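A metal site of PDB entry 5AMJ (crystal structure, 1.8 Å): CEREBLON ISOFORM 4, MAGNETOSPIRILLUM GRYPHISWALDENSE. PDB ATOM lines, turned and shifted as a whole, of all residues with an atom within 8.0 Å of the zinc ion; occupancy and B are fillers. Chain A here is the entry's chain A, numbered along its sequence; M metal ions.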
ATOM      1  N   ARG A  24     -16.789  17.093 -21.667  1.00  0.00           N
ATOM      2  CA  ARG A  24     -17.297  16.094 -22.591  1.00  0.00           C
ATOM      3  C   ARG A  24     -16.961  16.541 -23.984  1.00  0.00           C
ATOM      4  O   ARG A  24     -16.731  17.736 -24.302  1.00  0.00           O
ATOM      5  CB  ARG A  24     -18.832  16.007 -22.469  1.00  0.00           C
ATOM      6  CG  ARG A  24     -19.232  15.349 -21.175  1.00  0.00           C
ATOM      7  CD  ARG A  24     -20.742  15.176 -21.063  1.00  0.00           C
ATOM      8  NE  ARG A  24     -21.030  14.622 -19.763  1.00  0.00           N
ATOM      9  CZ  ARG A  24     -20.886  13.343 -19.455  1.00  0.00           C
ATOM     10  NH1 ARG A  24     -20.524  12.478 -20.378  1.00  0.00           N
ATOM     11  NH2 ARG A  24     -21.075  12.926 -18.211  1.00  0.00           N
ATOM     12  N   CYS A  25     -16.937  15.569 -24.889  1.00  0.00           N
ATOM     13  CA  CYS A  25     -16.833  15.908 -26.304  1.00  0.00           C
ATOM     14  C   CYS A  25     -17.962  16.768 -26.785  1.00  0.00           C
ATOM     15  O   CYS A  25     -19.133  16.403 -26.646  1.00  0.00           O
ATOM     16  CB  CYS A  25     -16.691  14.617 -27.196  1.00  0.00           C
ATOM     17  SG  CYS A  25     -16.715  14.888 -29.005  1.00  0.00           S
ATOM     18  N   ARG A  26     -17.666  17.891 -27.426  1.00  0.00           N
ATOM     19  CA  ARG A  26     -18.690  18.770 -27.862  1.00  0.00           C
ATOM     20  C   ARG A  26     -19.621  18.166 -28.967  1.00  0.00           C
ATOM     21  O   ARG A  26     -20.786  18.508 -29.102  1.00  0.00           O
ATOM     22  CB  ARG A  26     -18.059  20.060 -28.364  1.00  0.00           C
ATOM     23  CG  ARG A  26     -18.963  20.993 -29.083  1.00  0.00           C
ATOM     24  CD  ARG A  26     -18.223  22.239 -29.531  1.00  0.00           C
ATOM     25  NE  ARG A  26     -19.138  23.106 -30.223  1.00  0.00           N
ATOM     26  CZ  ARG A  26     -18.774  24.275 -30.766  1.00  0.00           C
ATOM     27  NH1 ARG A  26     -17.500  24.694 -30.669  1.00  0.00           N
ATOM     28  NH2 ARG A  26     -19.662  24.971 -31.410  1.00  0.00           N
ATOM     29  N   GLN A  27     -19.048  17.257 -29.741  1.00  0.00           N
ATOM     30  CA  GLN A  27     -19.743  16.721 -30.897  1.00  0.00           C
ATOM     31  C   GLN A  27     -20.623  15.567 -30.562  1.00  0.00           C
ATOM     32  O   GLN A  27     -21.620  15.354 -31.255  1.00  0.00           O
ATOM     33  CB  GLN A  27     -18.734  16.239 -31.930  1.00  0.00           C
ATOM     34  CG  GLN A  27     -17.953  17.354 -32.591  1.00  0.00           C
ATOM     35  CD  GLN A  27     -18.804  18.554 -32.907  1.00  0.00           C
ATOM     36  OE1 GLN A  27     -18.532  19.673 -32.420  1.00  0.00           O
ATOM     37  NE2 GLN A  27     -19.831  18.370 -33.718  1.00  0.00           N
ATOM     38  N   CYS A  28     -20.349  14.855 -29.460  1.00  0.00           N
ATOM     39  CA  CYS A  28     -21.181  13.674 -29.134  1.00  0.00           C
ATOM     40  C   CYS A  28     -21.468  13.429 -27.692  1.00  0.00           C
ATOM     41  O   CYS A  28     -22.381  12.689 -27.347  1.00  0.00           O
ATOM     42  CB  CYS A  28     -20.572  12.421 -29.708  1.00  0.00           C
ATOM     43  SG  CYS A  28     -19.099  11.837 -28.784  1.00  0.00           S
ATOM     44  N   GLY A  29     -20.794  14.124 -26.777  1.00  0.00           N
ATOM     45  CA  GLY A  29     -21.068  13.939 -25.378  1.00  0.00           C
ATOM     46  C   GLY A  29     -20.262  12.970 -24.593  1.00  0.00           C
ATOM     47  O   GLY A  29     -20.367  12.874 -23.365  1.00  0.00           O
ATOM     48  N   GLN A  30     -19.310  12.266 -25.247  1.00  0.00           N
ATOM     49  CA  GLN A  30     -18.445  11.344 -24.543  1.00  0.00           C
ATOM     50  C   GLN A  30     -17.689  12.001 -23.401  1.00  0.00           C
ATOM     51  O   GLN A  30     -17.178  13.085 -23.587  1.00  0.00           O
ATOM     52  CB  GLN A  30     -17.397  10.812 -25.523  1.00  0.00           C
ATOM     53  CG  GLN A  30     -16.312   9.956 -24.901  1.00  0.00           C
ATOM     54  CD  GLN A  30     -16.637   8.491 -24.862  1.00  0.00           C
ATOM     55  OE1 GLN A  30     -17.739   8.095 -24.525  1.00  0.00           O
ATOM     56  NE2 GLN A  30     -15.660   7.651 -25.251  1.00  0.00           N
ATOM     57  N   THR A  31     -17.614  11.342 -22.241  1.00  0.00           N
ATOM     58  CA  THR A  31     -16.894  11.879 -21.082  1.00  0.00           C
ATOM     59  C   THR A  31     -15.386  11.856 -21.380  1.00  0.00           C
ATOM     60  O   THR A  31     -14.854  10.807 -21.794  1.00  0.00           O
ATOM     61  CB  THR A  31     -17.138  11.030 -19.837  1.00  0.00           C
ATOM     62  OG1 THR A  31     -18.529  10.974 -19.569  1.00  0.00           O
ATOM     63  CG2 THR A  31     -16.582  11.753 -18.666  1.00  0.00           C
ATOM     64  N   ILE A  32     -14.719  12.986 -21.172  1.00  0.00           N
ATOM     65  CA  ILE A  32     -13.312  13.118 -21.549  1.00  0.00           C
ATOM     66  C   ILE A  32     -12.446  13.520 -20.318  1.00  0.00           C
ATOM     67  O   ILE A  32     -11.446  12.851 -20.055  1.00  0.00           O
ATOM     68  CB  ILE A  32     -13.065  14.143 -22.669  1.00  0.00           C
ATOM     69  CG1 ILE A  32     -13.848  13.822 -23.921  1.00  0.00           C
ATOM     70  CG2 ILE A  32     -11.579  14.253 -23.015  1.00  0.00           C
ATOM     71  CD1 ILE A  32     -13.475  12.519 -24.567  1.00  0.00           C
ATOM     72  N   GLY A  67     -11.782   8.184 -22.452  1.00  0.00           N
ATOM     73  CA  GLY A  67     -12.671   8.216 -23.567  1.00  0.00           C
ATOM     74  C   GLY A  67     -12.144   8.607 -24.895  1.00  0.00           C
ATOM     75  O   GLY A  67     -12.904   8.902 -25.798  1.00  0.00           O
ATOM     76  N   LEU A  68     -10.828   8.709 -24.986  1.00  0.00           N
ATOM     77  CA  LEU A  68     -10.122   9.077 -26.237  1.00  0.00           C
ATOM     78  C   LEU A  68      -9.643   7.841 -26.946  1.00  0.00           C
ATOM     79  O   LEU A  68      -9.685   6.749 -26.420  1.00  0.00           O
ATOM     80  CB  LEU A  68      -8.902  10.006 -25.932  1.00  0.00           C
ATOM     81  CG  LEU A  68      -9.314  11.345 -25.334  1.00  0.00           C
ATOM     82  CD1 LEU A  68      -8.085  11.924 -24.602  1.00  0.00           C
ATOM     83  CD2 LEU A  68      -9.918  12.315 -26.305  1.00  0.00           C
ATOM     84  N   LEU A  90      -8.166  11.347 -30.529  1.00  0.00           N
ATOM     85  CA  LEU A  90      -9.508  11.437 -31.047  1.00  0.00           C
ATOM     86  C   LEU A  90     -10.520  11.092 -29.946  1.00  0.00           C
ATOM     87  O   LEU A  90     -10.226  10.343 -29.044  1.00  0.00           O
ATOM     88  CB  LEU A  90      -9.763  10.475 -32.205  1.00  0.00           C
ATOM     89  CG  LEU A  90      -8.816  10.529 -33.402  1.00  0.00           C
ATOM     90  CD1 LEU A  90      -9.306   9.533 -34.405  1.00  0.00           C
ATOM     91  CD2 LEU A  90      -8.712  11.935 -33.964  1.00  0.00           C
ATOM     92  N   CYS A  91     -11.698  11.653 -30.094  1.00  0.00           N
ATOM     93  CA  CYS A  91     -12.834  11.128 -29.294  1.00  0.00           C
ATOM     94  C   CYS A  91     -12.999   9.678 -29.649  1.00  0.00           C
ATOM     95  O   CYS A  91     -13.132   9.312 -30.824  1.00  0.00           O
ATOM     96  CB  CYS A  91     -14.082  11.940 -29.586  1.00  0.00           C
ATOM     97  SG  CYS A  91     -15.550  11.292 -28.682  1.00  0.00           S
ATOM     98  N   GLY A  92     -12.991   8.827 -28.624  1.00  0.00           N
ATOM     99  CA  GLY A  92     -13.132   7.406 -28.826  1.00  0.00           C
ATOM    100  C   GLY A  92     -14.527   6.994 -29.312  1.00  0.00           C
ATOM    101  O   GLY A  92     -14.714   5.871 -29.785  1.00  0.00           O
ATOM    102  N   GLN A  93     -15.509   7.856 -29.103  1.00  0.00           N
ATOM    103  CA  GLN A  93     -16.869   7.545 -29.532  1.00  0.00           C
ATOM    104  C   GLN A  93     -17.099   8.053 -30.952  1.00  0.00           C
ATOM    105  O   GLN A  93     -17.523   7.270 -31.783  1.00  0.00           O
ATOM    106  CB  GLN A  93     -17.866   8.146 -28.518  1.00  0.00           C
ATOM    107  CG  GLN A  93     -19.325   7.939 -28.751  1.00  0.00           C
ATOM    108  CD  GLN A  93     -20.130   8.128 -27.467  1.00  0.00           C
ATOM    109  OE1 GLN A  93     -20.363   7.188 -26.742  1.00  0.00           O
ATOM    110  NE2 GLN A  93     -20.501   9.356 -27.158  1.00  0.00           N
ATOM    111  N   CYS A  94     -16.860   9.333 -31.237  1.00  0.00           N
ATOM    112  CA  CYS A  94     -17.220   9.907 -32.532  1.00  0.00           C
ATOM    113  C   CYS A  94     -16.101  10.134 -33.511  1.00  0.00           C
ATOM    114  O   CYS A  94     -16.394  10.402 -34.694  1.00  0.00           O
ATOM    115  CB  CYS A  94     -18.094  11.157 -32.407  1.00  0.00           C
ATOM    116  SG  CYS A  94     -17.106  12.613 -31.985  1.00  0.00           S
ATOM    117  N   GLY A  95     -14.887  10.023 -33.016  1.00  0.00           N
ATOM    118  CA  GLY A  95     -13.674  10.286 -33.816  1.00  0.00           C
ATOM    119  C   GLY A  95     -13.310  11.751 -34.052  1.00  0.00           C
ATOM    120  O   GLY A  95     -12.292  12.023 -34.747  1.00  0.00           O
ATOM    121  N   SER A  96     -14.034  12.692 -33.482  1.00  0.00           N
ATOM    122  CA  SER A  96     -13.608  14.142 -33.447  1.00  0.00           C
ATOM    123  C   SER A  96     -12.178  14.295 -32.954  1.00  0.00           C
ATOM    124  O   SER A  96     -11.757  13.673 -31.979  1.00  0.00           O
ATOM    125  CB  SER A  96     -14.576  15.018 -32.638  1.00  0.00           C
ATOM    126  OG  SER A  96     -14.190  16.393 -32.472  1.00  0.00           O
ATOM    127  N   HIS A  97     -11.420  15.150 -33.612  1.00  0.00           N
ATOM    128  CA  HIS A  97     -10.085  15.395 -33.140  1.00  0.00           C
ATOM    129  C   HIS A  97     -10.129  16.385 -31.936  1.00  0.00           C
ATOM    130  O   HIS A  97     -10.374  17.581 -32.096  1.00  0.00           O
ATOM    131  CB  HIS A  97      -9.196  15.895 -34.298  1.00  0.00           C
ATOM    132  CG  HIS A  97      -7.818  16.250 -33.827  1.00  0.00           C
ATOM    133  ND1 HIS A  97      -7.063  17.245 -34.402  1.00  0.00           N
ATOM    134  CD2 HIS A  97      -7.073  15.762 -32.812  1.00  0.00           C
ATOM    135  CE1 HIS A  97      -5.885  17.320 -33.797  1.00  0.00           C
ATOM    136  NE2 HIS A  97      -5.895  16.471 -32.789  1.00  0.00           N
ATOM    137  N   LEU A  98      -9.864  15.869 -30.741  1.00  0.00           N
ATOM    138  CA  LEU A  98      -9.947  16.618 -29.480  1.00  0.00           C
ATOM    139  C   LEU A  98      -8.629  17.218 -29.038  1.00  0.00           C
ATOM    140  O   LEU A  98      -8.611  18.214 -28.330  1.00  0.00           O
ATOM    141  CB  LEU A  98     -10.556  15.799 -28.346  1.00  0.00           C
ATOM    142  CG  LEU A  98     -11.976  15.334 -28.658  1.00  0.00           C
ATOM    143  CD1 LEU A  98     -12.544  14.739 -27.385  1.00  0.00           C
ATOM    144  CD2 LEU A  98     -12.873  16.460 -29.110  1.00  0.00           C
ATOM    145  N   ARG A 118     -13.477  22.382 -28.571  1.00  0.00           N
ATOM    146  CA  ARG A 118     -13.966  21.079 -28.997  1.00  0.00           C
ATOM    147  C   ARG A 118     -14.533  20.245 -27.840  1.00  0.00           C
ATOM    148  O   ARG A 118     -14.947  19.073 -28.023  1.00  0.00           O
ATOM    149  CB  ARG A 118     -12.888  20.313 -29.784  1.00  0.00           C
ATOM    150  CG  ARG A 118     -12.554  21.133 -31.019  1.00  0.00           C
ATOM    151  CD  ARG A 118     -11.675  20.318 -31.941  1.00  0.00           C
ATOM    152  NE  ARG A 118     -11.233  21.207 -33.005  1.00  0.00           N
ATOM    153  CZ  ARG A 118     -10.446  20.858 -34.011  1.00  0.00           C
ATOM    154  NH1 ARG A 118     -10.030  19.599 -34.100  1.00  0.00           N
ATOM    155  NH2 ARG A 118     -10.109  21.756 -34.946  1.00  0.00           N
HETATM  156 ZN    ZN M   1     -17.152  12.707 -29.645  1.00  0.00          ZN
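SG of Cys 28 sits close to N of Gln 30 (3.6 Å). NE2 of Gln 93 lies close to SG of Cys 28. SG of Cys 25 sits close to N of Gln 27 (3.4 Å). N of Cys 25 sits at hydrogen-bond distance from O of Gln 30, 2.8 Å away. SG of Cys 94 sits close to N of Ser 96, at 3.4 Å. N of Cys 91 lies within hydrogen-bond range of O of Ser 96 (2.8 Å). N of Gln 93 lies close to SG of Cys 91 (3.5 Å).
Within 4 Å of the zinc ion: Cys 25, Cys 28, Cys 91 and Cys 94. Along chain A the residues within 4 Å of the zinc ion span positions 25 to 94. The nearest printed residue that does not touch the zinc ion is Gln 27 (4.5 Å).
The zinc ion is bound by SG of Cys 28 (2.3 Å). The zinc ion is bound by SG of Cys 25. The side-chain sulfur (SG) of Cys 94 is bound to the zinc ion (2.3 Å). SG of Cys 91 is bound to the zinc ion (2.3 Å).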
